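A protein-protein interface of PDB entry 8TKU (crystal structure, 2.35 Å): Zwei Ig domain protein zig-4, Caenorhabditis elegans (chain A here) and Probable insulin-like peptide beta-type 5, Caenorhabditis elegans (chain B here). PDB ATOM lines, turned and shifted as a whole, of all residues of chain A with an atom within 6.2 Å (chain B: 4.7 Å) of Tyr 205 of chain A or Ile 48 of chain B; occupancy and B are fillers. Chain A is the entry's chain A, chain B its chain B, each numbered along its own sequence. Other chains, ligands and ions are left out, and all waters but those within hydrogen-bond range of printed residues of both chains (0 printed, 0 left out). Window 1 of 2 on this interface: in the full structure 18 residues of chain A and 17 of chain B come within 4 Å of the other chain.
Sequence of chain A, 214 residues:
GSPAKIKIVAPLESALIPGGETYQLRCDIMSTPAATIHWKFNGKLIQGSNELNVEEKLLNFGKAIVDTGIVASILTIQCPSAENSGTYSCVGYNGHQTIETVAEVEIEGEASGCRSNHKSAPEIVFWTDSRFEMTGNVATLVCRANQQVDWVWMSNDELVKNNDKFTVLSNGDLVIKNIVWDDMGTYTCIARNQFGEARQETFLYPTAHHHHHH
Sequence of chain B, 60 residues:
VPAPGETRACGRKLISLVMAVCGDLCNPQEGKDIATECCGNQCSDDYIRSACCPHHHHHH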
ATOM      1  N   ARG A 131      -3.273  17.119   1.509  1.00  0.00           N
ATOM      2  CA  ARG A 131      -2.147  18.036   1.490  1.00  0.00           C
ATOM      3  C   ARG A 131      -2.337  19.032   2.620  1.00  0.00           C
ATOM      4  O   ARG A 131      -3.413  19.620   2.774  1.00  0.00           O
ATOM      5  CB  ARG A 131      -2.011  18.739   0.146  1.00  0.00           C
ATOM      6  CG  ARG A 131      -1.129  19.991   0.184  1.00  0.00           C
ATOM      7  CD  ARG A 131       0.316  19.649   0.475  1.00  0.00           C
ATOM      8  NE  ARG A 131       1.108  20.860   0.627  1.00  0.00           N
ATOM      9  CZ  ARG A 131       1.675  21.543  -0.364  1.00  0.00           C
ATOM     10  NH1 ARG A 131       2.340  22.667  -0.131  1.00  0.00           N
ATOM     11  NH2 ARG A 131       1.579  21.091  -1.617  1.00  0.00           N
ATOM     12  N   PHE A 132      -1.313  19.163   3.442  1.00  0.00           N
ATOM     13  CA  PHE A 132      -1.297  20.088   4.558  1.00  0.00           C
ATOM     14  C   PHE A 132      -0.309  21.175   4.209  1.00  0.00           C
ATOM     15  O   PHE A 132       0.765  20.884   3.666  1.00  0.00           O
ATOM     16  CB  PHE A 132      -0.899  19.391   5.875  1.00  0.00           C
ATOM     17  CG  PHE A 132      -1.939  18.431   6.383  1.00  0.00           C
ATOM     18  CD1 PHE A 132      -2.111  17.195   5.785  1.00  0.00           C
ATOM     19  CD2 PHE A 132      -2.764  18.776   7.438  1.00  0.00           C
ATOM     20  CE1 PHE A 132      -3.100  16.316   6.237  1.00  0.00           C
ATOM     21  CE2 PHE A 132      -3.741  17.919   7.895  1.00  0.00           C
ATOM     22  CZ  PHE A 132      -3.914  16.683   7.293  1.00  0.00           C
ATOM     23  N   GLU A 133      -0.695  22.426   4.472  1.00  0.00           N
ATOM     24  CA  GLU A 133       0.188  23.544   4.184  1.00  0.00           C
ATOM     25  C   GLU A 133      -0.170  24.704   5.074  1.00  0.00           C
ATOM     26  O   GLU A 133      -1.309  24.831   5.520  1.00  0.00           O
ATOM     27  CB  GLU A 133       0.139  23.982   2.731  1.00  0.00           C
ATOM     28  CG  GLU A 133       1.228  25.005   2.416  1.00  0.00           C
ATOM     29  CD  GLU A 133       2.602  24.577   2.906  1.00  0.00           C
ATOM     30  OE1 GLU A 133       3.153  23.643   2.290  1.00  0.00           O
ATOM     31  OE2 GLU A 133       3.124  25.168   3.891  1.00  0.00           O
ATOM     32  N   MET A 134       0.825  25.520   5.371  1.00  0.00           N
ATOM     33  CA  MET A 134       0.590  26.643   6.258  1.00  0.00           C
ATOM     34  C   MET A 134      -0.182  27.767   5.560  1.00  0.00           C
ATOM     35  O   MET A 134       0.058  28.091   4.390  1.00  0.00           O
ATOM     36  CB  MET A 134       1.913  27.165   6.796  1.00  0.00           C
ATOM     37  CG  MET A 134       1.739  28.020   8.033  1.00  0.00           C
ATOM     38  SD  MET A 134       3.314  28.651   8.610  1.00  0.00           S
ATOM     39  CE  MET A 134       4.219  27.111   8.903  1.00  0.00           C
ATOM     40  N   ILE A 179      -3.230  30.501   0.849  1.00  0.00           N
ATOM     41  CA  ILE A 179      -4.324  29.717   1.381  1.00  0.00           C
ATOM     42  C   ILE A 179      -4.703  30.241   2.761  1.00  0.00           C
ATOM     43  O   ILE A 179      -3.866  30.759   3.510  1.00  0.00           O
ATOM     44  CB  ILE A 179      -3.952  28.221   1.399  1.00  0.00           C
ATOM     45  CG1 ILE A 179      -2.770  27.922   2.320  1.00  0.00           C
ATOM     46  CG2 ILE A 179      -3.612  27.753  -0.023  1.00  0.00           C
ATOM     47  CD1 ILE A 179      -2.326  26.436   2.272  1.00  0.00           C
ATOM     48  N   TRP A 181      -7.791  29.439   6.129  1.00  0.00           N
ATOM     49  CA  TRP A 181      -8.557  28.370   6.755  1.00  0.00           C
ATOM     50  C   TRP A 181      -9.826  28.027   5.999  1.00  0.00           C
ATOM     51  O   TRP A 181     -10.207  26.855   5.935  1.00  0.00           O
ATOM     52  CB  TRP A 181      -8.910  28.756   8.186  1.00  0.00           C
ATOM     53  CG  TRP A 181      -9.784  27.758   8.873  1.00  0.00           C
ATOM     54  CD1 TRP A 181     -11.035  27.973   9.366  1.00  0.00           C
ATOM     55  CD2 TRP A 181      -9.476  26.378   9.143  1.00  0.00           C
ATOM     56  NE1 TRP A 181     -11.525  26.820   9.934  1.00  0.00           N
ATOM     57  CE2 TRP A 181     -10.589  25.825   9.810  1.00  0.00           C
ATOM     58  CE3 TRP A 181      -8.372  25.563   8.887  1.00  0.00           C
ATOM     59  CZ2 TRP A 181     -10.630  24.492  10.226  1.00  0.00           C
ATOM     60  CZ3 TRP A 181      -8.412  24.240   9.307  1.00  0.00           C
ATOM     61  CH2 TRP A 181      -9.538  23.719   9.963  1.00  0.00           C
ATOM     62  N   ASP A 183     -10.240  27.814   2.928  1.00  0.00           N
ATOM     63  CA  ASP A 183      -9.969  26.942   1.798  1.00  0.00           C
ATOM     64  C   ASP A 183      -9.958  25.468   2.180  1.00  0.00           C
ATOM     65  O   ASP A 183      -9.864  24.622   1.286  1.00  0.00           O
ATOM     66  CB  ASP A 183      -8.640  27.315   1.158  1.00  0.00           C
ATOM     67  CG  ASP A 183      -8.644  28.719   0.605  1.00  0.00           C
ATOM     68  OD1 ASP A 183      -9.630  29.088  -0.071  1.00  0.00           O
ATOM     69  OD2 ASP A 183      -7.659  29.451   0.846  1.00  0.00           O
ATOM     70  N   MET A 184     -10.064  25.149   3.472  1.00  0.00           N
ATOM     71  CA  MET A 184     -10.037  23.767   3.914  1.00  0.00           C
ATOM     72  C   MET A 184     -11.222  23.008   3.332  1.00  0.00           C
ATOM     73  O   MET A 184     -12.325  23.550   3.194  1.00  0.00           O
ATOM     74  CB  MET A 184     -10.055  23.710   5.446  1.00  0.00           C
ATOM     75  CG  MET A 184      -9.837  22.316   6.058  1.00  0.00           C
ATOM     76  SD  MET A 184     -11.334  21.335   6.337  1.00  0.00           S
ATOM     77  CE  MET A 184     -11.890  21.993   7.913  1.00  0.00           C
ATOM     78  N   GLY A 185     -10.978  21.758   2.953  1.00  0.00           N
ATOM     79  CA  GLY A 185     -12.038  20.876   2.543  1.00  0.00           C
ATOM     80  C   GLY A 185     -11.631  20.060   1.339  1.00  0.00           C
ATOM     81  O   GLY A 185     -10.456  19.961   0.996  1.00  0.00           O
ATOM     82  N   PHE A 203      -7.908  16.543  -0.772  1.00  0.00           N
ATOM     83  CA  PHE A 203      -8.235  17.239   0.464  1.00  0.00           C
ATOM     84  C   PHE A 203      -7.108  18.199   0.823  1.00  0.00           C
ATOM     85  O   PHE A 203      -5.933  17.845   0.732  1.00  0.00           O
ATOM     86  CB  PHE A 203      -8.477  16.250   1.596  1.00  0.00           C
ATOM     87  CG  PHE A 203      -8.790  16.899   2.887  1.00  0.00           C
ATOM     88  CD1 PHE A 203     -10.071  17.349   3.149  1.00  0.00           C
ATOM     89  CD2 PHE A 203      -7.786  17.104   3.836  1.00  0.00           C
ATOM     90  CE1 PHE A 203     -10.368  17.983   4.352  1.00  0.00           C
ATOM     91  CE2 PHE A 203      -8.063  17.727   5.054  1.00  0.00           C
ATOM     92  CZ  PHE A 203      -9.361  18.175   5.316  1.00  0.00           C
ATOM     93  N   LEU A 204      -7.463  19.418   1.225  1.00  0.00           N
ATOM     94  CA  LEU A 204      -6.489  20.436   1.599  1.00  0.00           C
ATOM     95  C   LEU A 204      -6.738  20.885   3.028  1.00  0.00           C
ATOM     96  O   LEU A 204      -7.878  21.192   3.392  1.00  0.00           O
ATOM     97  CB  LEU A 204      -6.586  21.631   0.677  1.00  0.00           C
ATOM     98  CG  LEU A 204      -5.818  22.863   1.108  1.00  0.00           C
ATOM     99  CD1 LEU A 204      -4.324  22.677   0.889  1.00  0.00           C
ATOM    100  CD2 LEU A 204      -6.382  24.054   0.358  1.00  0.00           C
ATOM    101  N   TYR A 205      -5.682  20.930   3.834  1.00  0.00           N
ATOM    102  CA  TYR A 205      -5.808  21.441   5.198  1.00  0.00           C
ATOM    103  C   TYR A 205      -4.843  22.583   5.407  1.00  0.00           C
ATOM    104  O   TYR A 205      -3.628  22.340   5.527  1.00  0.00           O
ATOM    105  CB  TYR A 205      -5.545  20.366   6.236  1.00  0.00           C
ATOM    106  CG  TYR A 205      -5.856  20.802   7.651  1.00  0.00           C
ATOM    107  CD1 TYR A 205      -4.974  21.587   8.379  1.00  0.00           C
ATOM    108  CD2 TYR A 205      -7.043  20.422   8.261  1.00  0.00           C
ATOM    109  CE1 TYR A 205      -5.267  21.971   9.684  1.00  0.00           C
ATOM    110  CE2 TYR A 205      -7.337  20.796   9.557  1.00  0.00           C
ATOM    111  CZ  TYR A 205      -6.455  21.565  10.264  1.00  0.00           C
ATOM    112  OH  TYR A 205      -6.781  21.928  11.554  1.00  0.00           O
ATOM    113  N   PRO A 206      -5.326  23.836   5.448  1.00  0.00           N
ATOM    114  CA  PRO A 206      -4.457  24.968   5.807  1.00  0.00           C
ATOM    115  C   PRO A 206      -4.175  24.977   7.304  1.00  0.00           C
ATOM    116  O   PRO A 206      -5.068  25.178   8.134  1.00  0.00           O
ATOM    117  CB  PRO A 206      -5.269  26.196   5.359  1.00  0.00           C
ATOM    118  CG  PRO A 206      -6.327  25.651   4.432  1.00  0.00           C
ATOM    119  CD  PRO A 206      -6.634  24.280   4.948  1.00  0.00           C
ATOM    120  N   THR A 207      -2.930  24.720   7.660  1.00  0.00           N
ATOM    121  CA  THR A 207      -2.550  24.626   9.056  1.00  0.00           C
ATOM    122  C   THR A 207      -2.290  26.013   9.637  1.00  0.00           C
ATOM    123  O   THR A 207      -2.130  27.003   8.920  1.00  0.00           O
ATOM    124  CB  THR A 207      -1.325  23.739   9.205  1.00  0.00           C
ATOM    125  OG1 THR A 207      -0.219  24.370   8.547  1.00  0.00           O
ATOM    126  CG2 THR A 207      -1.587  22.383   8.557  1.00  0.00           C
ATOM    127  N   ALA A 208      -2.230  26.072  10.963  1.00  0.00           N
ATOM    128  CA  ALA A 208      -2.089  27.347  11.645  1.00  0.00           C
ATOM    129  C   ALA A 208      -0.690  27.930  11.491  1.00  0.00           C
ATOM    130  O   ALA A 208       0.312  27.212  11.508  1.00  0.00           O
ATOM    131  CB  ALA A 208      -2.408  27.182  13.126  1.00  0.00           C
ATOM    132  N   CYS B  10     -12.642  15.629   6.297  1.00  0.00           N
ATOM    133  CA  CYS B  10     -11.531  16.102   7.118  1.00  0.00           C
ATOM    134  C   CYS B  10     -11.117  15.111   8.219  1.00  0.00           C
ATOM    135  O   CYS B  10      -9.928  14.798   8.369  1.00  0.00           O
ATOM    136  CB  CYS B  10     -11.897  17.467   7.693  1.00  0.00           C
ATOM    137  SG  CYS B  10     -10.643  18.172   8.718  1.00  0.00           S
ATOM    138  N   LEU B  14      -7.365  13.512   8.379  1.00  0.00           N
ATOM    139  CA  LEU B  14      -6.414  13.748   9.462  1.00  0.00           C
ATOM    140  C   LEU B  14      -6.031  12.442  10.146  1.00  0.00           C
ATOM    141  O   LEU B  14      -4.864  12.219  10.496  1.00  0.00           O
ATOM    142  CB  LEU B  14      -7.015  14.710  10.482  1.00  0.00           C
ATOM    143  CG  LEU B  14      -6.566  16.149  10.338  1.00  0.00           C
ATOM    144  CD1 LEU B  14      -7.137  16.666   9.035  1.00  0.00           C
ATOM    145  CD2 LEU B  14      -7.131  16.928  11.491  1.00  0.00           C
ATOM    146  N   LEU B  17      -3.525  10.685   8.178  1.00  0.00           N
ATOM    147  CA  LEU B  17      -2.217  11.309   8.300  1.00  0.00           C
ATOM    148  C   LEU B  17      -1.583  10.967   9.634  1.00  0.00           C
ATOM    149  O   LEU B  17      -0.396  10.621   9.708  1.00  0.00           O
ATOM    150  CB  LEU B  17      -2.337  12.822   8.165  1.00  0.00           C
ATOM    151  CG  LEU B  17      -0.958  13.464   8.307  1.00  0.00           C
ATOM    152  CD1 LEU B  17      -0.210  13.341   6.984  1.00  0.00           C
ATOM    153  CD2 LEU B  17      -1.035  14.885   8.802  1.00  0.00           C
ATOM    154  N   VAL B  18      -2.362  11.085  10.705  1.00  0.00           N
ATOM    155  CA  VAL B  18      -1.833  10.846  12.043  1.00  0.00           C
ATOM    156  C   VAL B  18      -1.367   9.400  12.193  1.00  0.00           C
ATOM    157  O   VAL B  18      -0.267   9.140  12.692  1.00  0.00           O
ATOM    158  CB  VAL B  18      -2.881  11.236  13.094  1.00  0.00           C
ATOM    159  CG1 VAL B  18      -2.616  10.503  14.375  1.00  0.00           C
ATOM    160  CG2 VAL B  18      -2.804  12.747  13.317  1.00  0.00           C
ATOM    161  N   CYS B  38      -9.281  19.029  15.400  1.00  0.00           N
ATOM    162  CA  CYS B  38      -8.608  19.804  14.366  1.00  0.00           C
ATOM    163  C   CYS B  38      -9.444  20.009  13.117  1.00  0.00           C
ATOM    164  O   CYS B  38      -9.074  20.830  12.266  1.00  0.00           O
ATOM    165  CB  CYS B  38      -7.285  19.145  13.991  1.00  0.00           C
ATOM    166  SG  CYS B  38      -6.126  19.341  15.308  1.00  0.00           S
ATOM    167  N   ASN B  41     -11.458  23.276  14.433  1.00  0.00           N
ATOM    168  CA  ASN B  41     -10.648  24.473  14.600  1.00  0.00           C
ATOM    169  C   ASN B  41      -9.309  24.278  13.919  1.00  0.00           C
ATOM    170  O   ASN B  41      -8.782  23.163  13.854  1.00  0.00           O
ATOM    171  CB  ASN B  41     -10.433  24.824  16.071  1.00  0.00           C
ATOM    172  CG  ASN B  41     -11.692  24.681  16.876  1.00  0.00           C
ATOM    173  OD1 ASN B  41     -11.809  23.779  17.706  1.00  0.00           O
ATOM    174  ND2 ASN B  41     -12.673  25.547  16.602  1.00  0.00           N
ATOM    175  N   GLN B  42      -8.763  25.372  13.414  1.00  0.00           N
ATOM    176  CA  GLN B  42      -7.503  25.293  12.701  1.00  0.00           C
ATOM    177  C   GLN B  42      -6.387  24.963  13.686  1.00  0.00           C
ATOM    178  O   GLN B  42      -6.191  25.677  14.675  1.00  0.00           O
ATOM    179  CB  GLN B  42      -7.227  26.601  11.972  1.00  0.00           C
ATOM    180  CG  GLN B  42      -5.993  26.530  11.109  1.00  0.00           C
ATOM    181  CD  GLN B  42      -5.790  27.782  10.320  1.00  0.00           C
ATOM    182  OE1 GLN B  42      -5.883  28.873  10.865  1.00  0.00           O
ATOM    183  NE2 GLN B  42      -5.455  27.643   9.047  1.00  0.00           N
ATOM    184  N   CYS B  43      -5.711  23.838  13.459  1.00  0.00           N
ATOM    185  CA  CYS B  43      -4.549  23.430  14.239  1.00  0.00           C
ATOM    186  C   CYS B  43      -3.269  23.712  13.457  1.00  0.00           C
ATOM    187  O   CYS B  43      -3.284  23.875  12.237  1.00  0.00           O
ATOM    188  CB  CYS B  43      -4.619  21.937  14.589  1.00  0.00           C
ATOM    189  SG  CYS B  43      -6.068  21.382  15.556  1.00  0.00           S
ATOM    190  N   SER B  44      -2.152  23.754  14.173  1.00  0.00           N
ATOM    191  CA  SER B  44      -0.855  23.926  13.531  1.00  0.00           C
ATOM    192  C   SER B  44      -0.313  22.596  13.025  1.00  0.00           C
ATOM    193  O   SER B  44      -0.719  21.519  13.467  1.00  0.00           O
ATOM    194  CB  SER B  44       0.169  24.514  14.492  1.00  0.00           C
ATOM    195  OG  SER B  44       0.499  23.547  15.468  1.00  0.00           O
ATOM    196  N   ASP B  45       0.640  22.692  12.099  1.00  0.00           N
ATOM    197  CA  ASP B  45       1.356  21.509  11.637  1.00  0.00           C
ATOM    198  C   ASP B  45       1.999  20.776  12.811  1.00  0.00           C
ATOM    199  O   ASP B  45       1.958  19.541  12.905  1.00  0.00           O
ATOM    200  CB  ASP B  45       2.416  21.917  10.617  1.00  0.00           C
ATOM    201  CG  ASP B  45       3.453  20.828  10.391  1.00  0.00           C
ATOM    202  OD1 ASP B  45       3.054  19.727   9.950  1.00  0.00           O
ATOM    203  OD2 ASP B  45       4.662  21.058  10.651  1.00  0.00           O
ATOM    204  N   ASP B  46       2.604  21.540  13.714  1.00  0.00           N
ATOM    205  CA  ASP B  46       3.331  20.979  14.841  1.00  0.00           C
ATOM    206  C   ASP B  46       2.421  20.114  15.716  1.00  0.00           C
ATOM    207  O   ASP B  46       2.787  18.993  16.099  1.00  0.00           O
ATOM    208  CB  ASP B  46       3.924  22.165  15.603  1.00  0.00           C
ATOM    209  CG  ASP B  46       4.653  21.776  16.837  1.00  0.00           C
ATOM    210  OD1 ASP B  46       5.673  21.064  16.719  1.00  0.00           O
ATOM    211  OD2 ASP B  46       4.216  22.208  17.929  1.00  0.00           O
ATOM    212  N   TYR B  47       1.209  20.597  16.003  1.00  0.00           N
ATOM    213  CA  TYR B  47       0.271  19.835  16.826  1.00  0.00           C
ATOM    214  C   TYR B  47      -0.208  18.572  16.117  1.00  0.00           C
ATOM    215  O   TYR B  47      -0.220  17.486  16.707  1.00  0.00           O
ATOM    216  CB  TYR B  47      -0.923  20.707  17.206  1.00  0.00           C
ATOM    217  CG  TYR B  47      -1.934  20.020  18.108  1.00  0.00           C
ATOM    218  CD1 TYR B  47      -1.687  19.871  19.473  1.00  0.00           C
ATOM    219  CD2 TYR B  47      -3.127  19.517  17.600  1.00  0.00           C
ATOM    220  CE1 TYR B  47      -2.611  19.254  20.305  1.00  0.00           C
ATOM    221  CE2 TYR B  47      -4.056  18.897  18.426  1.00  0.00           C
ATOM    222  CZ  TYR B  47      -3.792  18.767  19.775  1.00  0.00           C
ATOM    223  OH  TYR B  47      -4.705  18.149  20.599  1.00  0.00           O
ATOM    224  N   ILE B  48      -0.641  18.708  14.857  1.00  0.00           N
ATOM    225  CA  ILE B  48      -1.233  17.582  14.136  1.00  0.00           C
ATOM    226  C   ILE B  48      -0.258  16.417  14.059  1.00  0.00           C
ATOM    227  O   ILE B  48      -0.625  15.267  14.316  1.00  0.00           O
ATOM    228  CB  ILE B  48      -1.702  18.025  12.739  1.00  0.00           C
ATOM    229  CG1 ILE B  48      -2.852  19.030  12.860  1.00  0.00           C
ATOM    230  CG2 ILE B  48      -2.141  16.827  11.902  1.00  0.00           C
ATOM    231  CD1 ILE B  48      -3.200  19.708  11.554  1.00  0.00           C
ATOM    232  N   ARG B  49       1.001  16.693  13.738  1.00  0.00           N
ATOM    233  CA  ARG B  49       1.935  15.600  13.534  1.00  0.00           C
ATOM    234  C   ARG B  49       2.389  14.945  14.839  1.00  0.00           C
ATOM    235  O   ARG B  49       2.734  13.757  14.829  1.00  0.00           O
ATOM    236  CB  ARG B  49       3.114  16.082  12.688  1.00  0.00           C
ATOM    237  CG  ARG B  49       2.747  16.107  11.182  1.00  0.00           C
ATOM    238  CD  ARG B  49       3.938  16.406  10.239  1.00  0.00           C
ATOM    239  NE  ARG B  49       4.543  17.699  10.526  1.00  0.00           N
ATOM    240  CZ  ARG B  49       5.588  17.873  11.320  1.00  0.00           C
ATOM    241  NH1 ARG B  49       6.202  16.847  11.887  1.00  0.00           N
ATOM    242  NH2 ARG B  49       6.009  19.109  11.577  1.00  0.00           N
ATOM    243  N   SER B  50       2.369  15.650  15.975  1.00  0.00           N
ATOM    244  CA  SER B  50       2.941  15.075  17.191  1.00  0.00           C
ATOM    245  C   SER B  50       1.934  14.818  18.303  1.00  0.00           C
ATOM    246  O   SER B  50       2.323  14.288  19.345  1.00  0.00           O
ATOM    247  CB  SER B  50       4.059  15.961  17.753  1.00  0.00           C
ATOM    248  OG  SER B  50       3.538  17.194  18.206  1.00  0.00           O
ATOM    249  N   ALA B  51       0.667  15.201  18.139  1.00  0.00           N
ATOM    250  CA  ALA B  51      -0.295  15.032  19.229  1.00  0.00           C
ATOM    251  C   ALA B  51      -0.498  13.561  19.590  1.00  0.00           C
ATOM    252  O   ALA B  51      -0.588  13.212  20.773  1.00  0.00           O
ATOM    253  CB  ALA B  51      -1.625  15.689  18.876  1.00  0.00           C
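OH of Tyr 205 of chain A lies within hydrogen-bond range of O of Asn 41 of chain B (3.3 Å).
The backbone carbonyl oxygen (O) of Cys 43 of chain B sits at hydrogen-bond distance from the backbone NH (N) of Ala 208 of chain A, at 2.7 Å.
The backbone NH of Cys 43 of chain B sits at hydrogen-bond distance from the side-chain hydroxyl of Tyr 205 of chain A, at 2.9 Å.
NE2 of Gln 42 of chain B is in hydrogen-bond range of O of Thr 207 of chain A, at 3.4 Å.
NE2 of Gln 42 of chain B sits at hydrogen-bond distance from O of Pro 206 of chain A, at 2.7 Å.
OH of Tyr 205 of chain A lies within hydrogen-bond range of O of Cys 38 of chain B (2.6 Å).
The backbone carbonyl oxygen of Arg 131 of chain A is in hydrogen-bond range of the backbone NH of Tyr 205 of chain A (2.8 Å).
The backbone carbonyl oxygen of Phe 203 of chain A lies within hydrogen-bond range of the backbone NH of Arg 131 of chain A, at 2.9 Å.
The backbone NH (N) of Tyr 47 of chain B sits at hydrogen-bond distance from the side-chain hydroxyl (OG) of Ser 44 of chain B (3.1 Å).
N of Glu 133 of chain A sits at hydrogen-bond distance from O of Tyr 205 of chain A (3.1 Å).
The backbone carbonyl oxygen (O) of Glu 133 of chain A is in hydrogen-bond range of the backbone NH (N) of Thr 207 of chain A, 2.7 Å away.
OG of Ser 44 of chain B sits close to N of Asp 46 of chain B (3.4 Å).
Phe 132 of chain A touches Leu 14 of chain B (CZ to CD1, 3.7 Å).
Phe 132 of chain A touches Leu 17 of chain B (CE1 to CD2, 3.6 Å).
Cys 38 of chain B touches Trp 181 of chain A (O to CH2, 3.7 Å).
Gln 42 of chain B touches Trp 181 of chain A.
Leu 14 of chain B touches Tyr 205 of chain A.
Tyr 205 of chain A touches Ile 48 of chain B.
Cys 43 of chain B touches Thr 207 of chain A (O to CA, 3.3 Å).
Thr 207 of chain A touches Asp 45 of chain B (CB to N, 3.7 Å).
Ala 208 of chain A touches Gln 42 of chain B (N to CG, 3.8 Å).
Ala 208 of chain A touches Ser 44 of chain B.
Printed residues of chain B within 4 Å of Phe 132 of chain A: Leu 14 and Leu 17.
Printed residues of chain B within 4 Å of Phe 203 of chain A: Cys 10.
Of chain B, only Leu 14 (3.8 Å), Cys 38 (2.6 Å), Asn 41 (3.3 Å), Gln 42 (3.6 Å), Cys 43 (2.9 Å) and Ile 48 (3.6 Å) come within 4 Å of Tyr 205 of chain A.
Of the printed residues of chain B, Thr 207 of chain A touches Gln 42, Cys 43 and Asp 45.
Of the printed residues of chain A, Leu 17 of chain B touches Phe 132.
Printed residues of chain A within 4 Å of Cys 38 of chain B: Trp 181 (3.7 Å) and Tyr 205 (2.6 Å).
Ile 48 of chain B touches one residue of chain A.
The nearest residue of chain B that does not touch Tyr 205 of chain A is Cys 10 of chain B (4.3 Å).
The nearest residue of chain A that does not touch Ile 48 of chain B is Phe 132 of chain A (4.1 Å).
The nearest printed residue of chain A that does not touch Cys 10 of chain B is Met 184 of chain A (4.02 Å).
Of the 16 printed residues of chain B, 10 touch a printed residue of chain A.
Along chain B the printed residues that touch a printed residue of chain A span positions 10 to 48.
Hydrophobic or aromatic side chains of chain A within 4 Å of the printed part of chain B: Phe 132, Trp 181, Phe 203, Tyr 205, Pro 206 and Ala 208.
Among the printed residues, no Asp or Glu carboxylate lies within 4 Å of a Lys or Arg side-chain nitrogen of the other chain.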
